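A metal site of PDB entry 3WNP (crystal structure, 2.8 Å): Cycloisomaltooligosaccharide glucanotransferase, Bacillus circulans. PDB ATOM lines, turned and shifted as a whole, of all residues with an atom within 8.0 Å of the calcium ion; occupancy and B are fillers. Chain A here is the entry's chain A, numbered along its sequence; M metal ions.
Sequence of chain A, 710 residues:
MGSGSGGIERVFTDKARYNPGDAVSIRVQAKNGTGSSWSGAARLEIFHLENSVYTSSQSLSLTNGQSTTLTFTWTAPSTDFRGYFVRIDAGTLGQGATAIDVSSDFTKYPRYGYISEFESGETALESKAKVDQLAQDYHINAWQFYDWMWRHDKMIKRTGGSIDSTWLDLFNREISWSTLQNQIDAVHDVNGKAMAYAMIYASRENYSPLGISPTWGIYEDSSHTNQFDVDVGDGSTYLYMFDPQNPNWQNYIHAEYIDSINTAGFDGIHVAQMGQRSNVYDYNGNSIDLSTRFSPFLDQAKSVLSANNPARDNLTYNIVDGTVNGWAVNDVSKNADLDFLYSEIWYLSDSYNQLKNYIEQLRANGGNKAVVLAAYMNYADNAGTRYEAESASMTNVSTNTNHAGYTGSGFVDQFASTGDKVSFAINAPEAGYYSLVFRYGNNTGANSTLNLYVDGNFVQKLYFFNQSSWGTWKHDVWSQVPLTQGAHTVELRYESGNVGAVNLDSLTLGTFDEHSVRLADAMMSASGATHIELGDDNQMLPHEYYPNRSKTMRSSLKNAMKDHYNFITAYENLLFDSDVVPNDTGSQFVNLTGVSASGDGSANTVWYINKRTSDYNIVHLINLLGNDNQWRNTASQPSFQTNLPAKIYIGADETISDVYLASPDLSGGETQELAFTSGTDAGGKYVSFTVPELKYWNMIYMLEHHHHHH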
ATOM      1  N   ARG A 386      16.055 -28.865 -14.632  1.00  0.00           N
ATOM      2  CA  ARG A 386      16.586 -28.028 -15.714  1.00  0.00           C
ATOM      3  C   ARG A 386      17.645 -27.084 -15.240  1.00  0.00           C
ATOM      4  O   ARG A 386      17.525 -26.484 -14.168  1.00  0.00           O
ATOM      5  CB  ARG A 386      15.477 -27.206 -16.339  1.00  0.00           C
ATOM      6  CG  ARG A 386      15.858 -26.512 -17.654  1.00  0.00           C
ATOM      7  CD  ARG A 386      14.606 -26.242 -18.518  1.00  0.00           C
ATOM      8  NE  ARG A 386      13.381 -26.275 -17.721  1.00  0.00           N
ATOM      9  CZ  ARG A 386      12.317 -25.525 -17.931  1.00  0.00           C
ATOM     10  NH1 ARG A 386      12.258 -24.686 -18.940  1.00  0.00           N
ATOM     11  NH2 ARG A 386      11.272 -25.657 -17.124  1.00  0.00           N
ATOM     12  N   TYR A 387      18.683 -26.975 -16.046  1.00  0.00           N
ATOM     13  CA  TYR A 387      19.743 -26.042 -15.804  1.00  0.00           C
ATOM     14  C   TYR A 387      19.734 -25.113 -17.027  1.00  0.00           C
ATOM     15  O   TYR A 387      20.054 -25.524 -18.149  1.00  0.00           O
ATOM     16  CB  TYR A 387      21.070 -26.773 -15.643  1.00  0.00           C
ATOM     17  CG  TYR A 387      21.260 -27.578 -14.348  1.00  0.00           C
ATOM     18  CD1 TYR A 387      21.788 -26.986 -13.206  1.00  0.00           C
ATOM     19  CD2 TYR A 387      20.983 -28.927 -14.294  1.00  0.00           C
ATOM     20  CE1 TYR A 387      21.994 -27.717 -12.033  1.00  0.00           C
ATOM     21  CE2 TYR A 387      21.179 -29.673 -13.136  1.00  0.00           C
ATOM     22  CZ  TYR A 387      21.688 -29.067 -12.008  1.00  0.00           C
ATOM     23  OH  TYR A 387      21.880 -29.824 -10.856  1.00  0.00           O
ATOM     24  N   GLU A 388      19.331 -23.865 -16.795  1.00  0.00           N
ATOM     25  CA  GLU A 388      19.185 -22.910 -17.875  1.00  0.00           C
ATOM     26  C   GLU A 388      20.525 -22.579 -18.502  1.00  0.00           C
ATOM     27  O   GLU A 388      21.483 -22.321 -17.801  1.00  0.00           O
ATOM     28  CB  GLU A 388      18.490 -21.649 -17.369  1.00  0.00           C
ATOM     29  CG  GLU A 388      16.990 -21.814 -17.043  1.00  0.00           C
ATOM     30  CD  GLU A 388      16.107 -22.271 -18.216  1.00  0.00           C
ATOM     31  OE1 GLU A 388      16.535 -22.208 -19.401  1.00  0.00           O
ATOM     32  OE2 GLU A 388      14.939 -22.678 -17.942  1.00  0.00           O
ATOM     33  N   ALA A 389      20.586 -22.568 -19.824  1.00  0.00           N
ATOM     34  CA  ALA A 389      21.839 -22.259 -20.531  1.00  0.00           C
ATOM     35  C   ALA A 389      22.329 -20.828 -20.319  1.00  0.00           C
ATOM     36  O   ALA A 389      23.501 -20.538 -20.433  1.00  0.00           O
ATOM     37  CB  ALA A 389      21.660 -22.532 -22.000  1.00  0.00           C
ATOM     38  N   GLU A 390      21.408 -19.933 -20.013  1.00  0.00           N
ATOM     39  CA  GLU A 390      21.741 -18.543 -19.811  1.00  0.00           C
ATOM     40  C   GLU A 390      22.040 -18.209 -18.320  1.00  0.00           C
ATOM     41  O   GLU A 390      22.466 -17.088 -18.000  1.00  0.00           O
ATOM     42  CB  GLU A 390      20.618 -17.660 -20.375  1.00  0.00           C
ATOM     43  CG  GLU A 390      19.287 -17.730 -19.636  1.00  0.00           C
ATOM     44  CD  GLU A 390      18.427 -18.929 -19.982  1.00  0.00           C
ATOM     45  OE1 GLU A 390      18.945 -19.944 -20.523  1.00  0.00           O
ATOM     46  OE2 GLU A 390      17.208 -18.858 -19.684  1.00  0.00           O
ATOM     47  N   SER A 391      21.796 -19.162 -17.430  1.00  0.00           N
ATOM     48  CA  SER A 391      22.320 -19.076 -16.057  1.00  0.00           C
ATOM     49  C   SER A 391      23.766 -19.572 -15.986  1.00  0.00           C
ATOM     50  O   SER A 391      24.469 -19.301 -15.031  1.00  0.00           O
ATOM     51  CB  SER A 391      21.469 -19.906 -15.092  1.00  0.00           C
ATOM     52  OG  SER A 391      20.206 -19.305 -14.878  1.00  0.00           O
ATOM     53  N   ASN A 400      20.471 -14.283 -25.718  1.00  0.00           N
ATOM     54  CA  ASN A 400      19.523 -13.467 -26.458  1.00  0.00           C
ATOM     55  C   ASN A 400      18.127 -13.868 -26.049  1.00  0.00           C
ATOM     56  O   ASN A 400      17.966 -14.688 -25.140  1.00  0.00           O
ATOM     57  CB  ASN A 400      19.715 -13.622 -27.954  1.00  0.00           C
ATOM     58  CG  ASN A 400      19.316 -12.366 -28.727  1.00  0.00           C
ATOM     59  OD1 ASN A 400      18.421 -11.606 -28.316  1.00  0.00           O
ATOM     60  ND2 ASN A 400      19.966 -12.145 -29.847  1.00  0.00           N
ATOM     61  N   GLY A 405       9.812 -19.270 -27.786  1.00  0.00           N
ATOM     62  CA  GLY A 405       9.551 -20.649 -27.334  1.00  0.00           C
ATOM     63  C   GLY A 405      10.579 -21.154 -26.341  1.00  0.00           C
ATOM     64  O   GLY A 405      10.418 -22.230 -25.749  1.00  0.00           O
ATOM     65  N   TYR A 406      11.644 -20.369 -26.151  1.00  0.00           N
ATOM     66  CA  TYR A 406      12.705 -20.697 -25.206  1.00  0.00           C
ATOM     67  C   TYR A 406      12.133 -20.648 -23.790  1.00  0.00           C
ATOM     68  O   TYR A 406      11.048 -20.116 -23.560  1.00  0.00           O
ATOM     69  CB  TYR A 406      13.883 -19.712 -25.339  1.00  0.00           C
ATOM     70  CG  TYR A 406      13.525 -18.293 -24.913  1.00  0.00           C
ATOM     71  CD1 TYR A 406      13.401 -17.975 -23.548  1.00  0.00           C
ATOM     72  CD2 TYR A 406      13.272 -17.293 -25.870  1.00  0.00           C
ATOM     73  CE1 TYR A 406      13.058 -16.689 -23.145  1.00  0.00           C
ATOM     74  CE2 TYR A 406      12.935 -16.006 -25.474  1.00  0.00           C
ATOM     75  CZ  TYR A 406      12.818 -15.707 -24.108  1.00  0.00           C
ATOM     76  OH  TYR A 406      12.475 -14.451 -23.669  1.00  0.00           O
ATOM     77  N   THR A 407      12.871 -21.197 -22.840  1.00  0.00           N
ATOM     78  CA  THR A 407      12.423 -21.256 -21.458  1.00  0.00           C
ATOM     79  C   THR A 407      13.332 -20.425 -20.545  1.00  0.00           C
ATOM     80  O   THR A 407      14.477 -20.082 -20.903  1.00  0.00           O
ATOM     81  CB  THR A 407      12.366 -22.715 -20.968  1.00  0.00           C
ATOM     82  OG1 THR A 407      13.687 -23.245 -20.758  1.00  0.00           O
ATOM     83  CG2 THR A 407      11.629 -23.609 -21.958  1.00  0.00           C
ATOM     84  N   GLY A 408      12.820 -20.136 -19.347  1.00  0.00           N
ATOM     85  CA  GLY A 408      13.408 -19.117 -18.487  1.00  0.00           C
ATOM     86  C   GLY A 408      13.570 -17.805 -19.244  1.00  0.00           C
ATOM     87  O   GLY A 408      12.726 -17.421 -20.042  1.00  0.00           O
ATOM     88  N   SER A 409      14.709 -17.155 -19.061  1.00  0.00           N
ATOM     89  CA  SER A 409      14.896 -15.779 -19.515  1.00  0.00           C
ATOM     90  C   SER A 409      15.454 -15.643 -20.939  1.00  0.00           C
ATOM     91  O   SER A 409      15.465 -14.541 -21.516  1.00  0.00           O
ATOM     92  CB  SER A 409      15.790 -15.023 -18.522  1.00  0.00           C
ATOM     93  OG  SER A 409      16.989 -15.729 -18.296  1.00  0.00           O
ATOM     94  N   GLY A 410      15.914 -16.751 -21.493  1.00  0.00           N
ATOM     95  CA  GLY A 410      16.473 -16.717 -22.843  1.00  0.00           C
ATOM     96  C   GLY A 410      17.274 -17.947 -23.205  1.00  0.00           C
ATOM     97  O   GLY A 410      16.936 -19.081 -22.835  1.00  0.00           O
ATOM     98  N   PHE A 411      18.342 -17.709 -23.943  1.00  0.00           N
ATOM     99  CA  PHE A 411      19.139 -18.780 -24.467  1.00  0.00           C
ATOM    100  C   PHE A 411      20.454 -18.220 -24.954  1.00  0.00           C
ATOM    101  O   PHE A 411      20.647 -17.002 -24.999  1.00  0.00           O
ATOM    102  CB  PHE A 411      18.397 -19.443 -25.642  1.00  0.00           C
ATOM    103  CG  PHE A 411      18.068 -18.518 -26.769  1.00  0.00           C
ATOM    104  CD1 PHE A 411      18.985 -18.279 -27.775  1.00  0.00           C
ATOM    105  CD2 PHE A 411      16.828 -17.902 -26.831  1.00  0.00           C
ATOM    106  CE1 PHE A 411      18.678 -17.449 -28.834  1.00  0.00           C
ATOM    107  CE2 PHE A 411      16.518 -17.063 -27.891  1.00  0.00           C
ATOM    108  CZ  PHE A 411      17.438 -16.833 -28.896  1.00  0.00           C
ATOM    109  N   VAL A 412      21.331 -19.132 -25.339  1.00  0.00           N
ATOM    110  CA  VAL A 412      22.635 -18.765 -25.849  1.00  0.00           C
ATOM    111  C   VAL A 412      22.602 -18.773 -27.372  1.00  0.00           C
ATOM    112  O   VAL A 412      22.192 -19.764 -27.958  1.00  0.00           O
ATOM    113  CB  VAL A 412      23.666 -19.775 -25.326  1.00  0.00           C
ATOM    114  CG1 VAL A 412      25.015 -19.537 -25.971  1.00  0.00           C
ATOM    115  CG2 VAL A 412      23.731 -19.704 -23.798  1.00  0.00           C
ATOM    116  N   ARG A 439      18.240 -28.856 -24.926  1.00  0.00           N
ATOM    117  CA  ARG A 439      17.234 -28.200 -25.768  1.00  0.00           C
ATOM    118  C   ARG A 439      17.911 -27.182 -26.682  1.00  0.00           C
ATOM    119  O   ARG A 439      18.626 -26.297 -26.209  1.00  0.00           O
ATOM    120  CB  ARG A 439      16.163 -27.519 -24.935  1.00  0.00           C
ATOM    121  CG  ARG A 439      14.931 -27.134 -25.717  1.00  0.00           C
ATOM    122  CD  ARG A 439      13.763 -26.869 -24.781  1.00  0.00           C
ATOM    123  NE  ARG A 439      12.473 -26.813 -25.468  1.00  0.00           N
ATOM    124  CZ  ARG A 439      11.808 -25.707 -25.798  1.00  0.00           C
ATOM    125  NH1 ARG A 439      12.277 -24.490 -25.509  1.00  0.00           N
ATOM    126  NH2 ARG A 439      10.645 -25.840 -26.440  1.00  0.00           N
ATOM    127  N   TRP A 473      12.325 -25.334 -31.558  1.00  0.00           N
ATOM    128  CA  TRP A 473      13.142 -25.924 -30.484  1.00  0.00           C
ATOM    129  C   TRP A 473      12.911 -27.416 -30.409  1.00  0.00           C
ATOM    130  O   TRP A 473      11.803 -27.881 -30.655  1.00  0.00           O
ATOM    131  CB  TRP A 473      12.816 -25.304 -29.136  1.00  0.00           C
ATOM    132  CG  TRP A 473      13.113 -23.839 -29.094  1.00  0.00           C
ATOM    133  CD1 TRP A 473      12.224 -22.830 -29.272  1.00  0.00           C
ATOM    134  CD2 TRP A 473      14.389 -23.226 -28.870  1.00  0.00           C
ATOM    135  NE1 TRP A 473      12.863 -21.619 -29.175  1.00  0.00           N
ATOM    136  CE2 TRP A 473      14.190 -21.830 -28.927  1.00  0.00           C
ATOM    137  CE3 TRP A 473      15.680 -23.712 -28.634  1.00  0.00           C
ATOM    138  CZ2 TRP A 473      15.222 -20.920 -28.749  1.00  0.00           C
ATOM    139  CZ3 TRP A 473      16.705 -22.805 -28.464  1.00  0.00           C
ATOM    140  CH2 TRP A 473      16.476 -21.430 -28.528  1.00  0.00           C
ATOM    141  N   LEU A 504      21.293 -22.528 -27.739  1.00  0.00           N
ATOM    142  CA  LEU A 504      21.209 -23.461 -26.639  1.00  0.00           C
ATOM    143  C   LEU A 504      20.333 -22.916 -25.547  1.00  0.00           C
ATOM    144  O   LEU A 504      20.513 -21.805 -25.100  1.00  0.00           O
ATOM    145  CB  LEU A 504      22.577 -23.771 -26.088  1.00  0.00           C
ATOM    146  CG  LEU A 504      22.584 -24.933 -25.090  1.00  0.00           C
ATOM    147  CD1 LEU A 504      22.076 -26.211 -25.740  1.00  0.00           C
ATOM    148  CD2 LEU A 504      23.992 -25.157 -24.549  1.00  0.00           C
ATOM    149  N   ASP A 505      19.371 -23.713 -25.146  1.00  0.00           N
ATOM    150  CA  ASP A 505      18.330 -23.241 -24.255  1.00  0.00           C
ATOM    151  C   ASP A 505      18.559 -23.785 -22.847  1.00  0.00           C
ATOM    152  O   ASP A 505      18.412 -23.072 -21.858  1.00  0.00           O
ATOM    153  CB  ASP A 505      16.960 -23.658 -24.822  1.00  0.00           C
ATOM    154  CG  ASP A 505      15.795 -22.952 -24.148  1.00  0.00           C
ATOM    155  OD1 ASP A 505      15.972 -21.809 -23.667  1.00  0.00           O
ATOM    156  OD2 ASP A 505      14.704 -23.534 -24.092  1.00  0.00           O
ATOM    157  N   SER A 506      18.947 -25.054 -22.739  1.00  0.00           N
ATOM    158  CA  SER A 506      19.058 -25.684 -21.446  1.00  0.00           C
ATOM    159  C   SER A 506      19.734 -27.033 -21.447  1.00  0.00           C
ATOM    160  O   SER A 506      19.916 -27.665 -22.508  1.00  0.00           O
ATOM    161  CB  SER A 506      17.668 -25.819 -20.785  1.00  0.00           C
ATOM    162  OG  SER A 506      16.665 -26.176 -21.703  1.00  0.00           O
ATOM    163  N   LEU A 507      20.158 -27.429 -20.251  1.00  0.00           N
ATOM    164  CA  LEU A 507      20.523 -28.802 -19.949  1.00  0.00           C
ATOM    165  C   LEU A 507      19.473 -29.296 -18.974  1.00  0.00           C
ATOM    166  O   LEU A 507      19.172 -28.612 -18.003  1.00  0.00           O
ATOM    167  CB  LEU A 507      21.924 -28.876 -19.313  1.00  0.00           C
ATOM    168  CG  LEU A 507      22.282 -30.166 -18.534  1.00  0.00           C
ATOM    169  CD1 LEU A 507      22.195 -31.423 -19.390  1.00  0.00           C
ATOM    170  CD2 LEU A 507      23.646 -30.010 -17.886  1.00  0.00           C
HETATM  171 CA    CA M   1      16.820 -21.049 -21.593  1.00  0.00          CA
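Five residues have an atom within 4 Å of the calcium ion: Glu 388, Glu 390, Thr 407, Gly 410 and Asp 505.
The nearest printed residue that does not touch the calcium ion is Phe 411 (4.3 Å).
The side-chain carboxylate (OE2) of Glu 388 is in salt-bridge range of the guanidinium group (NH1) of Arg 386, 3.5 Å away.
The guanidinium group of Arg 386 sits at hydrogen-bond distance from the side-chain hydroxyl of Thr 407, 2.7 Å away.
O of Asp 505 sits close to N of Ala 389 (3.0 Å).
The backbone NH (N) of Ser 409 is in hydrogen-bond range of the side-chain carboxylate (OE2) of Glu 390 (3.1 Å).
OD2 of Asp 505 lies within salt-bridge range of NH1 of Arg 439 (3.0 Å).
The backbone carbonyl oxygen (O) of Gly 410 is bound to the calcium ion, at 2.3 Å.
The side-chain carboxylate (OD1) of Asp 505 binds the calcium ion (2.4 Å).
OE1 of Glu 388 is bound to the calcium ion (2.5 Å).
O of Asp 505 is bound to the calcium ion, 2.6 Å away.
The calcium ion is bound by the side-chain carboxylate (OE1) of Glu 390.
The backbone carbonyl oxygen (O) of Thr 407 is bound to the calcium ion, at 2.6 Å.
The calcium ion has six donor atoms within binding distance.
Slightly farther from the calcium ion lies the side-chain carboxylate (OE2) of Glu 390 (2.9 Å).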
